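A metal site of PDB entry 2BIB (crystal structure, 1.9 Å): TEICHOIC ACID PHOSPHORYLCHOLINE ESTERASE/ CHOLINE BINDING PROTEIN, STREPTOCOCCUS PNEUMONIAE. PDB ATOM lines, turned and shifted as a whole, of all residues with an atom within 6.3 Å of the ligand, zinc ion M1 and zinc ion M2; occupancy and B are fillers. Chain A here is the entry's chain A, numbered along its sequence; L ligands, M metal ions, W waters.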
ATOM      1  N   GLY A  17       8.275 -32.232   6.772  1.00  0.00           N
ATOM      2  CA  GLY A  17       9.036 -31.052   6.436  1.00  0.00           C
ATOM      3  C   GLY A  17       9.628 -30.393   7.645  1.00  0.00           C
ATOM      4  O   GLY A  17       8.977 -30.269   8.685  1.00  0.00           O
ATOM      5  N   SER A  18      10.883 -29.953   7.496  1.00  0.00           N
ATOM      6  CA  SER A  18      11.615 -29.258   8.551  1.00  0.00           C
ATOM      7  C   SER A  18      12.875 -28.620   7.969  1.00  0.00           C
ATOM      8  O   SER A  18      13.513 -29.212   7.107  1.00  0.00           O
ATOM      9  CB  SER A  18      11.980 -30.231   9.696  1.00  0.00           C
ATOM     10  OG  SER A  18      12.690 -29.540  10.729  1.00  0.00           O
ATOM     11  N   ASP A  19      13.218 -27.433   8.468  1.00  0.00           N
ATOM     12  CA  ASP A  19      14.358 -26.649   7.972  1.00  0.00           C
ATOM     13  C   ASP A  19      15.489 -26.617   8.983  1.00  0.00           C
ATOM     14  O   ASP A  19      15.324 -26.100  10.075  1.00  0.00           O
ATOM     15  CB  ASP A  19      13.960 -25.195   7.740  1.00  0.00           C
ATOM     16  CG  ASP A  19      13.126 -24.975   6.491  1.00  0.00           C
ATOM     17  OD1 ASP A  19      12.422 -25.897   6.056  1.00  0.00           O
ATOM     18  OD2 ASP A  19      13.101 -23.857   5.897  1.00  0.00           O
ATOM     19  N   GLU A  36      13.474 -29.565  13.687  1.00  0.00           N
ATOM     20  CA  GLU A  36      12.668 -30.068  14.795  1.00  0.00           C
ATOM     21  C   GLU A  36      13.523 -30.732  15.862  1.00  0.00           C
ATOM     22  O   GLU A  36      14.494 -31.449  15.545  1.00  0.00           O
ATOM     23  CB  GLU A  36      11.615 -31.085  14.274  1.00  0.00           C
ATOM     24  CG  GLU A  36      10.602 -31.545  15.322  1.00  0.00           C
ATOM     25  CD  GLU A  36       9.738 -30.389  15.825  1.00  0.00           C
ATOM     26  OE1 GLU A  36       8.925 -29.882  15.025  1.00  0.00           O
ATOM     27  OE2 GLU A  36       9.889 -29.990  17.023  1.00  0.00           O
ATOM     28  N   GLY A  53      -1.673 -30.943  17.619  1.00  0.00           N
ATOM     29  CA  GLY A  53      -0.738 -30.694  16.541  1.00  0.00           C
ATOM     30  C   GLY A  53       0.717 -30.445  16.954  1.00  0.00           C
ATOM     31  O   GLY A  53       1.593 -30.419  16.088  1.00  0.00           O
ATOM     32  N   ILE A  54       0.986 -30.246  18.241  1.00  0.00           N
ATOM     33  CA  ILE A  54       2.382 -30.098  18.693  1.00  0.00           C
ATOM     34  C   ILE A  54       3.157 -31.373  18.309  1.00  0.00           C
ATOM     35  O   ILE A  54       2.694 -32.489  18.609  1.00  0.00           O
ATOM     36  CB  ILE A  54       2.477 -29.858  20.220  1.00  0.00           C
ATOM     37  CG1 ILE A  54       1.959 -28.457  20.604  1.00  0.00           C
ATOM     38  CG2 ILE A  54       3.916 -30.076  20.729  1.00  0.00           C
ATOM     39  CD1 ILE A  54       1.816 -28.257  22.115  1.00  0.00           C
ATOM     40  N   GLU A  55       4.310 -31.211  17.665  1.00  0.00           N
ATOM     41  CA  GLU A  55       5.147 -32.361  17.221  1.00  0.00           C
ATOM     42  C   GLU A  55       5.694 -33.237  18.374  1.00  0.00           C
ATOM     43  O   GLU A  55       6.320 -32.717  19.305  1.00  0.00           O
ATOM     44  CB  GLU A  55       6.320 -31.870  16.355  1.00  0.00           C
ATOM     45  CG  GLU A  55       7.122 -32.978  15.685  1.00  0.00           C
ATOM     46  CD  GLU A  55       6.269 -33.766  14.719  1.00  0.00           C
ATOM     47  OE1 GLU A  55       6.029 -33.270  13.598  1.00  0.00           O
ATOM     48  OE2 GLU A  55       5.804 -34.841  15.093  1.00  0.00           O
ATOM     49  N   HIS A  85      11.279 -18.208  11.927  1.00  0.00           N
ATOM     50  CA  HIS A  85      10.037 -18.045  12.680  1.00  0.00           C
ATOM     51  C   HIS A  85       9.985 -19.037  13.850  1.00  0.00           C
ATOM     52  O   HIS A  85      10.904 -19.825  14.017  1.00  0.00           O
ATOM     53  CB  HIS A  85       8.786 -18.125  11.757  1.00  0.00           C
ATOM     54  CG  HIS A  85       8.553 -19.456  11.098  1.00  0.00           C
ATOM     55  ND1 HIS A  85       9.485 -20.057  10.272  1.00  0.00           N
ATOM     56  CD2 HIS A  85       7.461 -20.266  11.101  1.00  0.00           C
ATOM     57  CE1 HIS A  85       8.973 -21.187   9.811  1.00  0.00           C
ATOM     58  NE2 HIS A  85       7.749 -21.344  10.297  1.00  0.00           N
ATOM     59  N   THR A  86       8.903 -19.033  14.631  1.00  0.00           N
ATOM     60  CA  THR A  86       8.879 -19.790  15.906  1.00  0.00           C
ATOM     61  C   THR A  86       8.360 -21.237  15.830  1.00  0.00           C
ATOM     62  O   THR A  86       8.269 -21.927  16.848  1.00  0.00           O
ATOM     63  CB  THR A  86       8.063 -19.012  16.960  1.00  0.00           C
ATOM     64  OG1 THR A  86       6.726 -18.802  16.473  1.00  0.00           O
ATOM     65  CG2 THR A  86       8.633 -17.590  17.165  1.00  0.00           C
ATOM     66  N   HIS A  87       8.024 -21.693  14.635  1.00  0.00           N
ATOM     67  CA  HIS A  87       7.558 -23.072  14.482  1.00  0.00           C
ATOM     68  C   HIS A  87       8.639 -24.076  14.885  1.00  0.00           C
ATOM     69  O   HIS A  87       9.805 -23.921  14.536  1.00  0.00           O
ATOM     70  CB  HIS A  87       7.012 -23.314  13.059  1.00  0.00           C
ATOM     71  CG  HIS A  87       5.711 -22.590  12.806  1.00  0.00           C
ATOM     72  ND1 HIS A  87       5.205 -22.373  11.535  1.00  0.00           N
ATOM     73  CD2 HIS A  87       4.832 -22.007  13.668  1.00  0.00           C
ATOM     74  CE1 HIS A  87       4.066 -21.696  11.634  1.00  0.00           C
ATOM     75  NE2 HIS A  87       3.819 -21.478  12.914  1.00  0.00           N
ATOM     76  N   SER A  88       8.239 -25.081  15.658  1.00  0.00           N
ATOM     77  CA  SER A  88       9.145 -26.053  16.242  1.00  0.00           C
ATOM     78  C   SER A  88      10.087 -26.688  15.209  1.00  0.00           C
ATOM     79  O   SER A  88      11.208 -27.051  15.533  1.00  0.00           O
ATOM     80  CB  SER A  88       8.346 -27.141  16.962  1.00  0.00           C
ATOM     81  OG  SER A  88       7.622 -27.927  16.031  1.00  0.00           O
ATOM     82  N   ASP A  89       9.629 -26.829  13.967  1.00  0.00           N
ATOM     83  CA  ASP A  89      10.411 -27.501  12.926  1.00  0.00           C
ATOM     84  C   ASP A  89      11.491 -26.594  12.312  1.00  0.00           C
ATOM     85  O   ASP A  89      12.214 -27.009  11.395  1.00  0.00           O
ATOM     86  CB  ASP A  89       9.519 -28.114  11.829  1.00  0.00           C
ATOM     87  CG  ASP A  89       8.666 -27.083  11.110  1.00  0.00           C
ATOM     88  OD1 ASP A  89       7.928 -26.356  11.806  1.00  0.00           O
ATOM     89  OD2 ASP A  89       8.664 -26.914   9.861  1.00  0.00           O
ATOM     90  N   HIS A  90      11.589 -25.372  12.850  1.00  0.00           N
ATOM     91  CA  HIS A  90      12.588 -24.371  12.466  1.00  0.00           C
ATOM     92  C   HIS A  90      13.442 -23.953  13.677  1.00  0.00           C
ATOM     93  O   HIS A  90      14.679 -24.017  13.620  1.00  0.00           O
ATOM     94  CB  HIS A  90      11.890 -23.168  11.832  1.00  0.00           C
ATOM     95  CG  HIS A  90      11.136 -23.535  10.587  1.00  0.00           C
ATOM     96  ND1 HIS A  90      11.623 -23.287   9.321  1.00  0.00           N
ATOM     97  CD2 HIS A  90       9.937 -24.150  10.406  1.00  0.00           C
ATOM     98  CE1 HIS A  90      10.754 -23.717   8.424  1.00  0.00           C
ATOM     99  NE2 HIS A  90       9.726 -24.253   9.051  1.00  0.00           N
ATOM    100  N   ARG A 121      -3.286 -22.199  15.685  1.00  0.00           N
ATOM    101  CA  ARG A 121      -1.951 -22.120  15.074  1.00  0.00           C
ATOM    102  C   ARG A 121      -0.920 -21.570  16.087  1.00  0.00           C
ATOM    103  O   ARG A 121       0.018 -20.839  15.729  1.00  0.00           O
ATOM    104  CB  ARG A 121      -2.009 -21.271  13.779  1.00  0.00           C
ATOM    105  CG  ARG A 121      -3.058 -21.801  12.722  1.00  0.00           C
ATOM    106  CD  ARG A 121      -2.920 -21.221  11.289  1.00  0.00           C
ATOM    107  NE  ARG A 121      -1.913 -21.969  10.514  1.00  0.00           N
ATOM    108  CZ  ARG A 121      -2.163 -23.052   9.765  1.00  0.00           C
ATOM    109  NH1 ARG A 121      -3.396 -23.532   9.630  1.00  0.00           N
ATOM    110  NH2 ARG A 121      -1.158 -23.656   9.145  1.00  0.00           N
ATOM    111  N   TRP A 123       0.223 -23.816  18.820  1.00  0.00           N
ATOM    112  CA  TRP A 123       1.022 -25.018  19.099  1.00  0.00           C
ATOM    113  C   TRP A 123       1.995 -24.782  20.285  1.00  0.00           C
ATOM    114  O   TRP A 123       1.579 -24.379  21.378  1.00  0.00           O
ATOM    115  CB  TRP A 123       1.769 -25.451  17.813  1.00  0.00           C
ATOM    116  CG  TRP A 123       0.826 -25.811  16.664  1.00  0.00           C
ATOM    117  CD1 TRP A 123      -0.097 -26.804  16.651  1.00  0.00           C
ATOM    118  CD2 TRP A 123       0.733 -25.156  15.378  1.00  0.00           C
ATOM    119  NE1 TRP A 123      -0.760 -26.827  15.443  1.00  0.00           N
ATOM    120  CE2 TRP A 123      -0.275 -25.826  14.642  1.00  0.00           C
ATOM    121  CE3 TRP A 123       1.402 -24.076  14.780  1.00  0.00           C
ATOM    122  CZ2 TRP A 123      -0.630 -25.449  13.334  1.00  0.00           C
ATOM    123  CZ3 TRP A 123       1.048 -23.708  13.477  1.00  0.00           C
ATOM    124  CH2 TRP A 123       0.036 -24.385  12.769  1.00  0.00           C
ATOM    125  N   ASP A 124       3.281 -25.039  20.037  1.00  0.00           N
ATOM    126  CA  ASP A 124       4.343 -24.723  20.994  1.00  0.00           C
ATOM    127  C   ASP A 124       5.307 -23.640  20.475  1.00  0.00           C
ATOM    128  O   ASP A 124       6.512 -23.694  20.735  1.00  0.00           O
ATOM    129  CB  ASP A 124       5.144 -25.978  21.344  1.00  0.00           C
ATOM    130  CG  ASP A 124       5.744 -26.669  20.124  1.00  0.00           C
ATOM    131  OD1 ASP A 124       5.348 -26.388  18.965  1.00  0.00           O
ATOM    132  OD2 ASP A 124       6.660 -27.500  20.257  1.00  0.00           O
ATOM    133  N   ASN A 125       4.757 -22.658  19.741  1.00  0.00           N
ATOM    134  CA  ASN A 125       5.547 -21.545  19.216  1.00  0.00           C
ATOM    135  C   ASN A 125       6.247 -20.789  20.366  1.00  0.00           C
ATOM    136  O   ASN A 125       7.440 -20.517  20.324  1.00  0.00           O
ATOM    137  CB  ASN A 125       4.678 -20.521  18.467  1.00  0.00           C
ATOM    138  CG  ASN A 125       3.934 -21.090  17.269  1.00  0.00           C
ATOM    139  OD1 ASN A 125       4.217 -22.192  16.794  1.00  0.00           O
ATOM    140  ND2 ASN A 125       2.941 -20.327  16.784  1.00  0.00           N
ATOM    141  N   ASP A 181      -0.649 -16.721  10.929  1.00  0.00           N
ATOM    142  CA  ASP A 181       0.259 -17.816  11.209  1.00  0.00           C
ATOM    143  C   ASP A 181       1.657 -17.203  11.193  1.00  0.00           C
ATOM    144  O   ASP A 181       1.921 -16.248  10.445  1.00  0.00           O
ATOM    145  CB  ASP A 181       0.122 -18.888  10.101  1.00  0.00           C
ATOM    146  CG  ASP A 181       1.018 -20.089  10.318  1.00  0.00           C
ATOM    147  OD1 ASP A 181       0.598 -21.090  10.959  1.00  0.00           O
ATOM    148  OD2 ASP A 181       2.165 -20.119   9.868  1.00  0.00           O
ATOM    149  N   ASP A 182       2.564 -17.715  12.024  1.00  0.00           N
ATOM    150  CA  ASP A 182       3.912 -17.146  12.064  1.00  0.00           C
ATOM    151  C   ASP A 182       4.720 -17.296  10.775  1.00  0.00           C
ATOM    152  O   ASP A 182       5.718 -16.606  10.578  1.00  0.00           O
ATOM    153  CB  ASP A 182       4.701 -17.698  13.244  1.00  0.00           C
ATOM    154  CG  ASP A 182       5.664 -16.684  13.805  1.00  0.00           C
ATOM    155  OD1 ASP A 182       6.738 -17.082  14.325  1.00  0.00           O
ATOM    156  OD2 ASP A 182       5.426 -15.455  13.750  1.00  0.00           O
ATOM    157  N   ASN A 183       4.294 -18.195   9.881  1.00  0.00           N
ATOM    158  CA  ASN A 183       4.937 -18.347   8.565  1.00  0.00           C
ATOM    159  C   ASN A 183       5.096 -17.019   7.809  1.00  0.00           C
ATOM    160  O   ASN A 183       6.112 -16.765   7.176  1.00  0.00           O
ATOM    161  CB  ASN A 183       4.151 -19.320   7.687  1.00  0.00           C
ATOM    162  CG  ASN A 183       4.354 -20.764   8.086  1.00  0.00           C
ATOM    163  OD1 ASN A 183       5.121 -21.067   9.016  1.00  0.00           O
ATOM    164  ND2 ASN A 183       3.660 -21.676   7.378  1.00  0.00           N
ATOM    165  N   SER A 186       8.221 -14.888   8.393  1.00  0.00           N
ATOM    166  CA  SER A 186       9.522 -15.487   8.084  1.00  0.00           C
ATOM    167  C   SER A 186      10.614 -14.495   7.682  1.00  0.00           C
ATOM    168  O   SER A 186      10.448 -13.705   6.740  1.00  0.00           O
ATOM    169  CB  SER A 186       9.409 -16.579   6.996  1.00  0.00           C
ATOM    170  OG  SER A 186       8.666 -17.678   7.474  1.00  0.00           O
ATOM    171  N   GLY A 202      12.540 -19.508   4.778  1.00  0.00           N
ATOM    172  CA  GLY A 202      11.773 -20.194   5.819  1.00  0.00           C
ATOM    173  C   GLY A 202      10.438 -20.715   5.324  1.00  0.00           C
ATOM    174  O   GLY A 202      10.387 -21.430   4.320  1.00  0.00           O
ATOM    175  N   ASP A 203       9.352 -20.320   6.001  1.00  0.00           N
ATOM    176  CA  ASP A 203       7.997 -20.799   5.669  1.00  0.00           C
ATOM    177  C   ASP A 203       7.178 -19.653   5.065  1.00  0.00           C
ATOM    178  O   ASP A 203       5.955 -19.644   5.144  1.00  0.00           O
ATOM    179  CB  ASP A 203       7.283 -21.441   6.921  1.00  0.00           C
ATOM    180  CG  ASP A 203       7.753 -22.879   7.226  1.00  0.00           C
ATOM    181  OD1 ASP A 203       7.383 -23.535   8.308  1.00  0.00           O
ATOM    182  OD2 ASP A 203       8.538 -23.430   6.402  1.00  0.00           O
ATOM    183  N   HIS A 228       7.983 -22.871   2.798  1.00  0.00           N
ATOM    184  CA  HIS A 228       7.031 -23.728   3.533  1.00  0.00           C
ATOM    185  C   HIS A 228       6.965 -25.175   2.998  1.00  0.00           C
ATOM    186  O   HIS A 228       5.870 -25.717   2.779  1.00  0.00           O
ATOM    187  CB  HIS A 228       5.635 -23.072   3.573  1.00  0.00           C
ATOM    188  CG  HIS A 228       4.656 -23.746   4.498  1.00  0.00           C
ATOM    189  ND1 HIS A 228       3.310 -23.770   4.236  1.00  0.00           N
ATOM    190  CD2 HIS A 228       4.833 -24.361   5.690  1.00  0.00           C
ATOM    191  CE1 HIS A 228       2.685 -24.413   5.216  1.00  0.00           C
ATOM    192  NE2 HIS A 228       3.584 -24.764   6.111  1.00  0.00           N
ATOM    193  N   HIS A 229       8.145 -25.756   2.749  1.00  0.00           N
ATOM    194  CA  HIS A 229       8.339 -27.198   2.533  1.00  0.00           C
ATOM    195  C   HIS A 229       7.782 -27.763   1.216  1.00  0.00           C
ATOM    196  O   HIS A 229       8.544 -28.354   0.429  1.00  0.00           O
ATOM    197  CB  HIS A 229       7.823 -28.033   3.743  1.00  0.00           C
ATOM    198  CG  HIS A 229       8.345 -27.539   5.066  1.00  0.00           C
ATOM    199  ND1 HIS A 229       9.661 -27.717   5.470  1.00  0.00           N
ATOM    200  CD2 HIS A 229       7.732 -26.870   6.063  1.00  0.00           C
ATOM    201  CE1 HIS A 229       9.818 -27.181   6.665  1.00  0.00           C
ATOM    202  NE2 HIS A 229       8.671 -26.657   7.051  1.00  0.00           N
HETATM  203  P1  LIG L   1       4.838 -25.400   9.329  1.00  0.00           P
HETATM  204  O1  LIG L   1       3.788 -26.198   8.412  1.00  0.00           O
HETATM  205  O2  LIG L   1       6.238 -26.016   8.967  1.00  0.00           O
HETATM  206  O3  LIG L   1       4.696 -23.862   9.146  1.00  0.00           O
HETATM  207  O4  LIG L   1       4.508 -25.749  10.872  1.00  0.00           O
HETATM  208  C1  LIG L   1       3.666 -26.876  11.096  1.00  0.00           C
HETATM  209  C2  LIG L   1       3.038 -26.775  12.481  1.00  0.00           C
HETATM  210  N1  LIG L   1       3.905 -27.291  13.563  1.00  0.00           N
HETATM  211  C3  LIG L   1       3.078 -28.145  14.420  1.00  0.00           C
HETATM  212  C4  LIG L   1       4.363 -26.142  14.360  1.00  0.00           C
HETATM  213  C5  LIG L   1       5.090 -28.058  13.085  1.00  0.00           C
HETATM  214 ZN    ZN M   1       8.092 -25.453   8.627  1.00  0.00          ZN
HETATM  215 ZN    ZN M   2       6.164 -22.605   9.689  1.00  0.00          ZN
HETATM  216  O   HOH W   1       1.686 -23.237   9.513  1.00  0.00           O
HETATM  217  O   HOH W   2       6.653 -28.849   8.807  1.00  0.00           O
HETATM  218  O   HOH W   3       5.125 -28.501  17.227  1.00  0.00           O
HETATM  219  O   HOH W   4       5.611 -24.572  16.948  1.00  0.00           O
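Residues that only touch the ligand: Gly 53 (3.2 Å), Ser 88 (3.9 Å) and Trp 123 (3.6 Å). Of the 25 residues printed, 10 come within 4 Å of the ligand.
Four residues have an atom within 4 Å of zinc ion M1: Asp 89, His 90, Asp 203 and His 229. The nearest printed residue that does not touch zinc ion M1 is His 85 (4.4 Å).
Zinc ion M2 is bound by OD1 of Asn 183 (2.0 Å), O3 of the ligand (2.0 Å), OD1 of Asp 203 (2.1 Å), ND1 of His 87 (2.1 Å) and NE2 of His 85 (2.1 Å).
Of the 25 residues printed, 5 come within 4 Å of zinc ion M2.
A ring nitrogen (NE2) of His 228 lies within hydrogen-bond range of an oxygen (O1) of the ligand (2.7 Å).
Zinc ion M1 is bound by O2 of the ligand (2.0 Å), OD2 of Asp 89 (2.0 Å), NE2 of His 229 (2.1 Å), OD1 of Asp 203 (2.1 Å) and NE2 of His 90 (2.1 Å).
Water W1 lies within hydrogen-bond range of OD1 of Asp 181 (2.8 Å), NH2 of Arg 121 (2.9 Å) and ND2 of Asn 183 (3.3 Å). Water W4 lies within hydrogen-bond range of OD1 of Asp 124 (2.7 Å), OD1 of Asn 125 (2.8 Å) and N of Ser 88 (3.0 Å). Water W3 lies within hydrogen-bond range of the side-chain carboxylate of Asp 124, the side-chain hydroxyl of Ser 88 and the backbone NH of Glu 55.
The side-chain amide nitrogen (ND2) of Asn 183 lies within hydrogen-bond range of a ring nitrogen (NE2) of His 228 (3.3 Å). The backbone NH (N) of Asn 183 lies within hydrogen-bond range of the side-chain carboxylate (OD2) of Asp 181 (2.9 Å). N of Asp 89 is in hydrogen-bond range of OE1 of Glu 36. O of Asp 89 sits at hydrogen-bond distance from N of Asp 19 (3.1 Å). The backbone NH (N) of Asp 203 is in hydrogen-bond range of the side-chain hydroxyl (OG) of Ser 186 (3.1 Å). The side-chain carboxylate (OD1) of Asp 19 lies close to a ring nitrogen (ND1) of His 229, at 3.4 Å. N of His 228 is in hydrogen-bond range of O of Gly 202. OG of Ser 88 sits at hydrogen-bond distance from OE1 of Glu 36 (2.6 Å).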
